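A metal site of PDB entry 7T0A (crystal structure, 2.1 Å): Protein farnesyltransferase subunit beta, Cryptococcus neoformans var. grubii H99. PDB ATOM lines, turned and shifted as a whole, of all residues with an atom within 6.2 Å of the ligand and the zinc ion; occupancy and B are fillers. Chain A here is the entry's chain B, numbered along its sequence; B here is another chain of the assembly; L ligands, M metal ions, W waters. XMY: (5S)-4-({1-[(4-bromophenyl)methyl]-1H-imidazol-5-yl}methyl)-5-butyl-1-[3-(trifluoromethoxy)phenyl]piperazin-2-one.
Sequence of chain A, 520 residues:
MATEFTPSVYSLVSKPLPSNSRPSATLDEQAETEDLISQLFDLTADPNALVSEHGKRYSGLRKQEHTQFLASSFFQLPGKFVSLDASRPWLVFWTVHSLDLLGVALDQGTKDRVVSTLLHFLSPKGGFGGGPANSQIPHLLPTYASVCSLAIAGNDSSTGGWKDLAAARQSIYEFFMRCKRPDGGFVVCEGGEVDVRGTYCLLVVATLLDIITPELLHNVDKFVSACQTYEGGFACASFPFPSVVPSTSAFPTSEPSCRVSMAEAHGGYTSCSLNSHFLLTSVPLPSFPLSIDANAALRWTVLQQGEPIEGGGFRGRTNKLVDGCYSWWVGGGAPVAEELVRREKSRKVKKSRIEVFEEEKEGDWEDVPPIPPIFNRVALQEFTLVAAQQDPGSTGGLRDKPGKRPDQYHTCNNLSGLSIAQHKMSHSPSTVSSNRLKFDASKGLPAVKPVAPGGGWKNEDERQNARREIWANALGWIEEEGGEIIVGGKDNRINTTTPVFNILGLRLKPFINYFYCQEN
F35 of the ligand sits close to SG of Cys 201 (3.1 Å). SG of Cys 272 sits close to F36 of the ligand (2.9 Å). Merely in contact with the ligand: Leu 84 (3.8 Å), Trp 90 (3.4 Å), Trp 94 (3.96 Å), Leu 141 (3.4 Å), Tyr 200 (3.4 Å), His 266 (3.4 Å), Gly 268 (3.5 Å), Tyr 269 (3.99 Å), Tyr 326 (3.3 Å), Trp 329 (3.5 Å) and Tyr 409 (3.4 Å). Within 4 Å of the ligand: Leu 84, Trp 90, Trp 94, Leu 141, Arg 197, Tyr 200, Cys 201, His 266, Gly 268, Tyr 269, Cys 272, Asp 323, Cys 325, Tyr 326, Trp 329, Tyr 409, His 410 and Tyr 123 of chain B.
The side-chain carboxylate (OD1) of Asp 407 is in hydrogen-bond range of the backbone NH (N) of His 410 (2.6 Å). OH of Tyr 409 lies close to SG of Cys 325 (3.2 Å). SG of Cys 272 sits at hydrogen-bond distance from O of Gly 268, 3.4 Å away. The side-chain hydroxyl of Tyr 123 of chain B lies within hydrogen-bond range of the side-chain hydroxyl of Tyr 269 (3.1 Å). The backbone carbonyl oxygen of Arg 197 lies within hydrogen-bond range of the side-chain sulfur of Cys 201, 3.3 Å away. A ring nitrogen (NE2) of His 266 lies within hydrogen-bond range of the side-chain hydroxyl of Tyr 326, 3.0 Å away. The side-chain hydroxyl (OH) of Tyr 200 is in hydrogen-bond range of the side-chain hydroxyl (OH) of Tyr 144 (3.2 Å). The side-chain hydroxyl (OH) of Tyr 409 lies within hydrogen-bond range of the indole nitrogen (NE1) of Trp 329, at 2.7 Å.
OH of Tyr 123 of chain B lies within hydrogen-bond range of O09 of the ligand. The guanidinium group (NH1) of Arg 197 is in hydrogen-bond range of an oxygen (O09) of the ligand.
Residues that only touch the zinc ion: Tyr 409 (3.9 Å). Within 4 Å of the zinc ion: Asp 323, Cys 325, Tyr 409 and His 410. The nearest printed residue that does not touch the zinc ion is Asp 400 (4.4 Å).
A nitrogen (N15) of the ligand is bound to the zinc ion, 2.2 Å away. A ring nitrogen (NE2) of His 410 is bound to the zinc ion (2.3 Å). SG of Cys 325 is bound to the zinc ion (2.3 Å). OD1 of Asp 323 binds the zinc ion (2.4 Å). The zinc ion is bound by OD2 of Asp 323, 2.5 Å away.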
ATOM      1  N   LEU A  84      12.134  -1.647   2.150  1.00  0.00           N
ATOM      2  CA  LEU A  84      12.697  -2.049   0.864  1.00  0.00           C
ATOM      3  C   LEU A  84      13.535  -0.957   0.231  1.00  0.00           C
ATOM      4  O   LEU A  84      13.851  -1.041  -0.963  1.00  0.00           O
ATOM      5  CB  LEU A  84      11.573  -2.480  -0.090  1.00  0.00           C
ATOM      6  CG  LEU A  84      10.749  -3.680   0.362  1.00  0.00           C
ATOM      7  CD1 LEU A  84       9.606  -3.934  -0.605  1.00  0.00           C
ATOM      8  CD2 LEU A  84      11.624  -4.922   0.490  1.00  0.00           C
ATOM      9  N   TRP A  90      15.652  -4.775  -6.704  1.00  0.00           N
ATOM     10  CA  TRP A  90      14.770  -5.949  -6.700  1.00  0.00           C
ATOM     11  C   TRP A  90      13.346  -5.551  -7.060  1.00  0.00           C
ATOM     12  O   TRP A  90      12.639  -6.312  -7.738  1.00  0.00           O
ATOM     13  CB  TRP A  90      14.824  -6.643  -5.346  1.00  0.00           C
ATOM     14  CG  TRP A  90      16.090  -7.387  -5.130  1.00  0.00           C
ATOM     15  CD1 TRP A  90      17.121  -7.028  -4.307  1.00  0.00           C
ATOM     16  CD2 TRP A  90      16.485  -8.619  -5.753  1.00  0.00           C
ATOM     17  NE1 TRP A  90      18.133  -7.954  -4.385  1.00  0.00           N
ATOM     18  CE2 TRP A  90      17.760  -8.946  -5.262  1.00  0.00           C
ATOM     19  CE3 TRP A  90      15.876  -9.464  -6.681  1.00  0.00           C
ATOM     20  CZ2 TRP A  90      18.446 -10.092  -5.669  1.00  0.00           C
ATOM     21  CZ3 TRP A  90      16.553 -10.607  -7.068  1.00  0.00           C
ATOM     22  CH2 TRP A  90      17.820 -10.910  -6.565  1.00  0.00           C
ATOM     23  N   TRP A  94      11.676  -7.553 -10.097  1.00  0.00           N
ATOM     24  CA  TRP A  94      10.388  -8.207  -9.889  1.00  0.00           C
ATOM     25  C   TRP A  94       9.317  -7.607 -10.777  1.00  0.00           C
ATOM     26  O   TRP A  94       8.386  -8.314 -11.196  1.00  0.00           O
ATOM     27  CB  TRP A  94       9.984  -8.106  -8.420  1.00  0.00           C
ATOM     28  CG  TRP A  94      10.866  -8.883  -7.492  1.00  0.00           C
ATOM     29  CD1 TRP A  94      11.556 -10.043  -7.777  1.00  0.00           C
ATOM     30  CD2 TRP A  94      11.177  -8.566  -6.127  1.00  0.00           C
ATOM     31  NE1 TRP A  94      12.261 -10.453  -6.679  1.00  0.00           N
ATOM     32  CE2 TRP A  94      12.050  -9.567  -5.650  1.00  0.00           C
ATOM     33  CE3 TRP A  94      10.804  -7.535  -5.270  1.00  0.00           C
ATOM     34  CZ2 TRP A  94      12.550  -9.569  -4.349  1.00  0.00           C
ATOM     35  CZ3 TRP A  94      11.307  -7.527  -3.969  1.00  0.00           C
ATOM     36  CH2 TRP A  94      12.171  -8.546  -3.527  1.00  0.00           C
ATOM     37  N   LEU A 141      23.649  -8.684  -4.084  1.00  0.00           N
ATOM     38  CA  LEU A 141      22.289  -9.018  -4.489  1.00  0.00           C
ATOM     39  C   LEU A 141      21.681  -7.945  -5.387  1.00  0.00           C
ATOM     40  O   LEU A 141      21.107  -8.302  -6.438  1.00  0.00           O
ATOM     41  CB  LEU A 141      21.417  -9.301  -3.261  1.00  0.00           C
ATOM     42  CG  LEU A 141      21.412 -10.737  -2.720  1.00  0.00           C
ATOM     43  CD1 LEU A 141      22.814 -11.222  -2.368  1.00  0.00           C
ATOM     44  CD2 LEU A 141      20.497 -10.846  -1.502  1.00  0.00           C
ATOM     45  N   TYR A 144      23.101  -8.352  -9.006  1.00  0.00           N
ATOM     46  CA  TYR A 144      22.370  -9.282  -9.853  1.00  0.00           C
ATOM     47  C   TYR A 144      21.072  -8.661 -10.361  1.00  0.00           C
ATOM     48  O   TYR A 144      20.776  -8.710 -11.560  1.00  0.00           O
ATOM     49  CB  TYR A 144      22.072 -10.576  -9.092  1.00  0.00           C
ATOM     50  CG  TYR A 144      20.990 -11.438  -9.709  1.00  0.00           C
ATOM     51  CD1 TYR A 144      21.312 -12.440 -10.623  1.00  0.00           C
ATOM     52  CD2 TYR A 144      19.651 -11.270  -9.377  1.00  0.00           C
ATOM     53  CE1 TYR A 144      20.329 -13.221 -11.203  1.00  0.00           C
ATOM     54  CE2 TYR A 144      18.670 -12.042  -9.943  1.00  0.00           C
ATOM     55  CZ  TYR A 144      19.005 -13.027 -10.849  1.00  0.00           C
ATOM     56  OH  TYR A 144      18.016 -13.796 -11.408  1.00  0.00           O
ATOM     57  N   VAL A 196      24.996 -18.519   0.229  1.00  0.00           N
ATOM     58  CA  VAL A 196      24.970 -18.915  -1.166  1.00  0.00           C
ATOM     59  C   VAL A 196      24.163 -17.973  -2.055  1.00  0.00           C
ATOM     60  O   VAL A 196      24.259 -18.075  -3.280  1.00  0.00           O
ATOM     61  CB  VAL A 196      24.401 -20.345  -1.313  1.00  0.00           C
ATOM     62  CG1 VAL A 196      25.379 -21.353  -0.724  1.00  0.00           C
ATOM     63  CG2 VAL A 196      23.045 -20.451  -0.635  1.00  0.00           C
ATOM     64  N   ARG A 197      23.382 -17.061  -1.474  1.00  0.00           N
ATOM     65  CA  ARG A 197      22.738 -16.040  -2.297  1.00  0.00           C
ATOM     66  C   ARG A 197      23.779 -15.146  -2.944  1.00  0.00           C
ATOM     67  O   ARG A 197      23.660 -14.792  -4.127  1.00  0.00           O
ATOM     68  CB  ARG A 197      21.774 -15.194  -1.457  1.00  0.00           C
ATOM     69  CG  ARG A 197      20.626 -15.944  -0.818  1.00  0.00           C
ATOM     70  CD  ARG A 197      19.912 -15.008   0.154  1.00  0.00           C
ATOM     71  NE  ARG A 197      20.872 -14.392   1.063  1.00  0.00           N
ATOM     72  CZ  ARG A 197      20.644 -13.283   1.757  1.00  0.00           C
ATOM     73  NH1 ARG A 197      19.478 -12.650   1.640  1.00  0.00           N
ATOM     74  NH2 ARG A 197      21.588 -12.798   2.553  1.00  0.00           N
ATOM     75  N   GLY A 198      24.800 -14.751  -2.180  1.00  0.00           N
ATOM     76  CA  GLY A 198      25.867 -13.952  -2.758  1.00  0.00           C
ATOM     77  C   GLY A 198      26.645 -14.697  -3.827  1.00  0.00           C
ATOM     78  O   GLY A 198      26.993 -14.127  -4.864  1.00  0.00           O
ATOM     79  N   TYR A 200      25.467 -17.152  -5.746  1.00  0.00           N
ATOM     80  CA  TYR A 200      24.615 -17.251  -6.926  1.00  0.00           C
ATOM     81  C   TYR A 200      24.579 -15.945  -7.703  1.00  0.00           C
ATOM     82  O   TYR A 200      24.791 -15.929  -8.919  1.00  0.00           O
ATOM     83  CB  TYR A 200      23.200 -17.661  -6.517  1.00  0.00           C
ATOM     84  CG  TYR A 200      22.163 -17.389  -7.585  1.00  0.00           C
ATOM     85  CD1 TYR A 200      22.057 -18.217  -8.693  1.00  0.00           C
ATOM     86  CD2 TYR A 200      21.304 -16.305  -7.487  1.00  0.00           C
ATOM     87  CE1 TYR A 200      21.115 -17.968  -9.672  1.00  0.00           C
ATOM     88  CE2 TYR A 200      20.364 -16.047  -8.466  1.00  0.00           C
ATOM     89  CZ  TYR A 200      20.270 -16.879  -9.558  1.00  0.00           C
ATOM     90  OH  TYR A 200      19.333 -16.633 -10.529  1.00  0.00           O
ATOM     91  N   CYS A 201      24.314 -14.834  -7.007  1.00  0.00           N
ATOM     92  CA  CYS A 201      24.229 -13.545  -7.675  1.00  0.00           C
ATOM     93  C   CYS A 201      25.542 -13.169  -8.336  1.00  0.00           C
ATOM     94  O   CYS A 201      25.562 -12.632  -9.444  1.00  0.00           O
ATOM     95  CB  CYS A 201      23.803 -12.465  -6.675  1.00  0.00           C
ATOM     96  SG  CYS A 201      22.092 -12.615  -6.113  1.00  0.00           S
ATOM     97  N   HIS A 266      16.978 -25.543   2.616  1.00  0.00           N
ATOM     98  CA  HIS A 266      15.980 -24.511   2.394  1.00  0.00           C
ATOM     99  C   HIS A 266      15.779 -24.304   0.901  1.00  0.00           C
ATOM    100  O   HIS A 266      16.737 -24.375   0.126  1.00  0.00           O
ATOM    101  CB  HIS A 266      16.401 -23.195   3.069  1.00  0.00           C
ATOM    102  CG  HIS A 266      15.361 -22.119   3.005  1.00  0.00           C
ATOM    103  ND1 HIS A 266      15.246 -21.270   1.932  1.00  0.00           N
ATOM    104  CD2 HIS A 266      14.392 -21.770   3.878  1.00  0.00           C
ATOM    105  CE1 HIS A 266      14.243 -20.423   2.148  1.00  0.00           C
ATOM    106  NE2 HIS A 266      13.715 -20.709   3.321  1.00  0.00           N
ATOM    107  N   GLY A 267      14.526 -24.051   0.514  1.00  0.00           N
ATOM    108  CA  GLY A 267      14.213 -23.964  -0.904  1.00  0.00           C
ATOM    109  C   GLY A 267      14.963 -22.872  -1.624  1.00  0.00           C
ATOM    110  O   GLY A 267      15.450 -23.070  -2.746  1.00  0.00           O
ATOM    111  N   GLY A 268      15.078 -21.691  -1.001  1.00  0.00           N
ATOM    112  CA  GLY A 268      15.802 -20.601  -1.639  1.00  0.00           C
ATOM    113  C   GLY A 268      17.288 -20.877  -1.752  1.00  0.00           C
ATOM    114  O   GLY A 268      17.896 -20.662  -2.800  1.00  0.00           O
ATOM    115  N   TYR A 269      17.894 -21.379  -0.669  1.00  0.00           N
ATOM    116  CA  TYR A 269      19.337 -21.641  -0.695  1.00  0.00           C
ATOM    117  C   TYR A 269      19.665 -22.890  -1.502  1.00  0.00           C
ATOM    118  O   TYR A 269      20.773 -23.006  -2.031  1.00  0.00           O
ATOM    119  CB  TYR A 269      19.860 -21.769   0.733  1.00  0.00           C
ATOM    120  CG  TYR A 269      19.593 -20.532   1.568  1.00  0.00           C
ATOM    121  CD1 TYR A 269      20.206 -19.322   1.264  1.00  0.00           C
ATOM    122  CD2 TYR A 269      18.738 -20.575   2.656  1.00  0.00           C
ATOM    123  CE1 TYR A 269      19.971 -18.190   2.021  1.00  0.00           C
ATOM    124  CE2 TYR A 269      18.493 -19.450   3.419  1.00  0.00           C
ATOM    125  CZ  TYR A 269      19.108 -18.263   3.094  1.00  0.00           C
ATOM    126  OH  TYR A 269      18.867 -17.128   3.843  1.00  0.00           O
ATOM    127  N   CYS A 272      19.814 -21.442  -5.052  1.00  0.00           N
ATOM    128  CA  CYS A 272      21.072 -20.726  -5.259  1.00  0.00           C
ATOM    129  C   CYS A 272      22.246 -21.687  -5.353  1.00  0.00           C
ATOM    130  O   CYS A 272      23.151 -21.495  -6.169  1.00  0.00           O
ATOM    131  CB  CYS A 272      21.299 -19.718  -4.127  1.00  0.00           C
ATOM    132  SG  CYS A 272      20.092 -18.374  -4.082  1.00  0.00           S
ATOM    133  N   ASP A 323       4.355 -22.260   0.127  1.00  0.00           N
ATOM    134  CA  ASP A 323       4.490 -20.841  -0.172  1.00  0.00           C
ATOM    135  C   ASP A 323       4.633 -20.691  -1.683  1.00  0.00           C
ATOM    136  O   ASP A 323       5.425 -21.394  -2.303  1.00  0.00           O
ATOM    137  CB  ASP A 323       5.707 -20.228   0.545  1.00  0.00           C
ATOM    138  CG  ASP A 323       5.773 -18.713   0.414  1.00  0.00           C
ATOM    139  OD1 ASP A 323       6.071 -18.057   1.434  1.00  0.00           O
ATOM    140  OD2 ASP A 323       5.520 -18.175  -0.681  1.00  0.00           O
ATOM    141  N   GLY A 324       3.858 -19.765  -2.255  1.00  0.00           N
ATOM    142  CA  GLY A 324       3.870 -19.601  -3.702  1.00  0.00           C
ATOM    143  C   GLY A 324       5.221 -19.209  -4.260  1.00  0.00           C
ATOM    144  O   GLY A 324       5.549 -19.563  -5.396  1.00  0.00           O
ATOM    145  N   CYS A 325       6.031 -18.486  -3.477  1.00  0.00           N
ATOM    146  CA  CYS A 325       7.326 -18.043  -3.979  1.00  0.00           C
ATOM    147  C   CYS A 325       8.287 -19.204  -4.199  1.00  0.00           C
ATOM    148  O   CYS A 325       9.204 -19.080  -5.004  1.00  0.00           O
ATOM    149  CB  CYS A 325       7.948 -17.024  -3.025  1.00  0.00           C
ATOM    150  SG  CYS A 325       8.585 -17.712  -1.478  1.00  0.00           S
ATOM    151  N   TYR A 326       8.078 -20.337  -3.524  1.00  0.00           N
ATOM    152  CA  TYR A 326       8.915 -21.507  -3.744  1.00  0.00           C
ATOM    153  C   TYR A 326       8.551 -22.263  -5.010  1.00  0.00           C
ATOM    154  O   TYR A 326       9.203 -23.261  -5.325  1.00  0.00           O
ATOM    155  CB  TYR A 326       8.848 -22.443  -2.532  1.00  0.00           C
ATOM    156  CG  TYR A 326       9.442 -21.831  -1.286  1.00  0.00           C
ATOM    157  CD1 TYR A 326      10.796 -21.501  -1.223  1.00  0.00           C
ATOM    158  CD2 TYR A 326       8.664 -21.562  -0.169  1.00  0.00           C
ATOM    159  CE1 TYR A 326      11.342 -20.934  -0.081  1.00  0.00           C
ATOM    160  CE2 TYR A 326       9.197 -20.991   0.971  1.00  0.00           C
ATOM    161  CZ  TYR A 326      10.534 -20.676   1.004  1.00  0.00           C
ATOM    162  OH  TYR A 326      11.081 -20.109   2.132  1.00  0.00           O
ATOM    163  N   TRP A 329      11.738 -21.082  -6.545  1.00  0.00           N
ATOM    164  CA  TRP A 329      12.944 -21.556  -5.852  1.00  0.00           C
ATOM    165  C   TRP A 329      13.076 -23.063  -5.970  1.00  0.00           C
ATOM    166  O   TRP A 329      14.130 -23.576  -6.388  1.00  0.00           O
ATOM    167  CB  TRP A 329      12.907 -21.139  -4.379  1.00  0.00           C
ATOM    168  CG  TRP A 329      12.950 -19.652  -4.141  1.00  0.00           C
ATOM    169  CD1 TRP A 329      12.053 -18.913  -3.420  1.00  0.00           C
ATOM    170  CD2 TRP A 329      13.939 -18.721  -4.625  1.00  0.00           C
ATOM    171  NE1 TRP A 329      12.428 -17.593  -3.426  1.00  0.00           N
ATOM    172  CE2 TRP A 329      13.578 -17.445  -4.156  1.00  0.00           C
ATOM    173  CE3 TRP A 329      15.086 -18.858  -5.406  1.00  0.00           C
ATOM    174  CZ2 TRP A 329      14.323 -16.304  -4.438  1.00  0.00           C
ATOM    175  CZ3 TRP A 329      15.838 -17.719  -5.693  1.00  0.00           C
ATOM    176  CH2 TRP A 329      15.445 -16.464  -5.206  1.00  0.00           C
ATOM    177  N   ASP A 400       1.903 -15.193  -1.270  1.00  0.00           N
ATOM    178  CA  ASP A 400       2.398 -16.382  -0.588  1.00  0.00           C
ATOM    179  C   ASP A 400       1.296 -17.428  -0.448  1.00  0.00           C
ATOM    180  O   ASP A 400       1.401 -18.550  -0.963  1.00  0.00           O
ATOM    181  CB  ASP A 400       2.967 -15.975   0.774  1.00  0.00           C
ATOM    182  CG  ASP A 400       3.173 -17.141   1.745  1.00  0.00           C
ATOM    183  OD1 ASP A 400       3.082 -18.322   1.359  1.00  0.00           O
ATOM    184  OD2 ASP A 400       3.436 -16.846   2.933  1.00  0.00           O
ATOM    185  N   ASP A 407       2.508  -9.181  -3.071  1.00  0.00           N
ATOM    186  CA  ASP A 407       3.601  -8.238  -3.195  1.00  0.00           C
ATOM    187  C   ASP A 407       4.344  -8.502  -4.501  1.00  0.00           C
ATOM    188  O   ASP A 407       4.082  -9.482  -5.202  1.00  0.00           O
ATOM    189  CB  ASP A 407       4.559  -8.304  -1.998  1.00  0.00           C
ATOM    190  CG  ASP A 407       5.013  -9.717  -1.692  1.00  0.00           C
ATOM    191  OD1 ASP A 407       5.651 -10.343  -2.559  1.00  0.00           O
ATOM    192  OD2 ASP A 407       4.757 -10.194  -0.569  1.00  0.00           O
ATOM    193  N   TYR A 409       7.463  -9.325  -4.939  1.00  0.00           N
ATOM    194  CA  TYR A 409       8.328 -10.487  -4.871  1.00  0.00           C
ATOM    195  C   TYR A 409       7.560 -11.772  -5.137  1.00  0.00           C
ATOM    196  O   TYR A 409       7.976 -12.607  -5.959  1.00  0.00           O
ATOM    197  CB  TYR A 409       9.026 -10.549  -3.504  1.00  0.00           C
ATOM    198  CG  TYR A 409       9.548 -11.924  -3.148  1.00  0.00           C
ATOM    199  CD1 TYR A 409      10.676 -12.448  -3.779  1.00  0.00           C
ATOM    200  CD2 TYR A 409       8.933 -12.696  -2.172  1.00  0.00           C
ATOM    201  CE1 TYR A 409      11.164 -13.694  -3.451  1.00  0.00           C
ATOM    202  CE2 TYR A 409       9.410 -13.949  -1.838  1.00  0.00           C
ATOM    203  CZ  TYR A 409      10.529 -14.438  -2.478  1.00  0.00           C
ATOM    204  OH  TYR A 409      10.998 -15.688  -2.138  1.00  0.00           O
ATOM    205  N   HIS A 410       6.423 -11.966  -4.453  1.00  0.00           N
ATOM    206  CA  HIS A 410       5.639 -13.172  -4.673  1.00  0.00           C
ATOM    207  C   HIS A 410       4.965 -13.171  -6.036  1.00  0.00           C
ATOM    208  O   HIS A 410       4.695 -14.235  -6.601  1.00  0.00           O
ATOM    209  CB  HIS A 410       4.599 -13.330  -3.567  1.00  0.00           C
ATOM    210  CG  HIS A 410       5.189 -13.714  -2.247  1.00  0.00           C
ATOM    211  ND1 HIS A 410       5.563 -12.777  -1.297  1.00  0.00           N
ATOM    212  CD2 HIS A 410       5.482 -14.926  -1.714  1.00  0.00           C
ATOM    213  CE1 HIS A 410       6.055 -13.398  -0.238  1.00  0.00           C
ATOM    214  NE2 HIS A 410       6.022 -14.708  -0.471  1.00  0.00           N
ATOM    215  N   TYR B 123      18.166  -9.404   8.045  1.00  0.00           N
ATOM    216  CA  TYR B 123      19.456 -10.034   7.827  1.00  0.00           C
ATOM    217  C   TYR B 123      20.576  -9.227   8.478  1.00  0.00           C
ATOM    218  O   TYR B 123      21.554  -9.788   8.985  1.00  0.00           O
ATOM    219  CB  TYR B 123      19.737 -10.175   6.324  1.00  0.00           C
ATOM    220  CG  TYR B 123      19.062 -11.339   5.639  1.00  0.00           C
ATOM    221  CD1 TYR B 123      19.663 -12.599   5.609  1.00  0.00           C
ATOM    222  CD2 TYR B 123      17.840 -11.188   5.009  1.00  0.00           C
ATOM    223  CE1 TYR B 123      19.055 -13.659   4.978  1.00  0.00           C
ATOM    224  CE2 TYR B 123      17.227 -12.247   4.370  1.00  0.00           C
ATOM    225  CZ  TYR B 123      17.833 -13.487   4.355  1.00  0.00           C
ATOM    226  OH  TYR B 123      17.221 -14.536   3.730  1.00  0.00           O
HETATM  227  C10 XMY L   1      13.794 -13.495   2.208  1.00  0.00           C
HETATM  228  C13 XMY L   1      10.678 -15.020   2.201  1.00  0.00           C
HETATM  229  C20 XMY L   1      14.555 -17.038   2.375  1.00  0.00           C
HETATM  230  C21 XMY L   1      15.630 -17.107   1.513  1.00  0.00           C
HETATM  231  C22 XMY L   1      15.424 -17.229   0.163  1.00  0.00           C
HETATM  232  C24 XMY L   1      14.120 -17.284  -0.322  1.00  0.00           C
HETATM  233  C26 XMY L   1      15.419 -12.776  -1.381  1.00  0.00           C
HETATM  234  C28 XMY L   1      17.192 -13.569  -2.838  1.00  0.00           C
HETATM  235  C01 XMY L   1      10.025  -8.359  -0.104  1.00  0.00           C
HETATM  236  C02 XMY L   1      11.270  -9.214   0.276  1.00  0.00           C
HETATM  237  C03 XMY L   1      10.920 -10.663   0.509  1.00  0.00           C
HETATM  238  C04 XMY L   1      12.088 -11.452   1.170  1.00  0.00           C
HETATM  239  C05 XMY L   1      12.144 -13.002   0.675  1.00  0.00           C
HETATM  240  C06 XMY L   1      13.019 -13.091  -0.529  1.00  0.00           C
HETATM  241  C08 XMY L   1      14.925 -13.230   1.102  1.00  0.00           C
HETATM  242  C12 XMY L   1      11.683 -13.905   2.625  1.00  0.00           C
HETATM  243  C14 XMY L   1       9.449 -14.825   1.626  1.00  0.00           C
HETATM  244  C16 XMY L   1       9.783 -16.979   1.831  1.00  0.00           C
HETATM  245  C18 XMY L   1      12.076 -17.003   2.897  1.00  0.00           C
HETATM  246  C19 XMY L   1      13.260 -17.087   1.898  1.00  0.00           C
HETATM  247  C25 XMY L   1      13.048 -17.206   0.540  1.00  0.00           C
HETATM  248  C27 XMY L   1      16.322 -13.808  -1.817  1.00  0.00           C
HETATM  249  C29 XMY L   1      17.196 -12.312  -3.453  1.00  0.00           C
HETATM  250  C30 XMY L   1      16.314 -11.309  -3.028  1.00  0.00           C
HETATM  251  C31 XMY L   1      15.432 -11.554  -1.987  1.00  0.00           C
HETATM  252  C33 XMY L   1      18.902 -14.422  -4.442  1.00  0.00           C
HETATM  253  F34 XMY L   1      18.116 -14.175  -5.538  1.00  0.00           F
HETATM  254  F35 XMY L   1      19.778 -13.365  -4.243  1.00  0.00           F
HETATM  255  F36 XMY L   1      19.625 -15.553  -4.667  1.00  0.00           F
HETATM  256  N07 XMY L   1      14.463 -13.039  -0.278  1.00  0.00           N
HETATM  257  N11 XMY L   1      12.570 -13.822   1.703  1.00  0.00           N
HETATM  258  N15 XMY L   1       8.904 -16.040   1.404  1.00  0.00           N
HETATM  259  N17 XMY L   1      10.874 -16.351   2.313  1.00  0.00           N
HETATM  260  O09 XMY L   1      16.034 -13.198   1.380  1.00  0.00           O
HETATM  261  O32 XMY L   1      18.098 -14.633  -3.258  1.00  0.00           O
HETATM  262 BR23 XMY L   1      16.957 -17.336  -1.053  1.00  0.00          BR
HETATM  263 ZN    ZN M   1       7.278 -16.565   0.021  1.00  0.00          ZN
HETATM  264  O   HOH W   1      13.125 -18.615   5.658  1.00  0.00           O
HETATM  265  O   HOH W   2       7.879  -7.372  -2.601  1.00  0.00           O
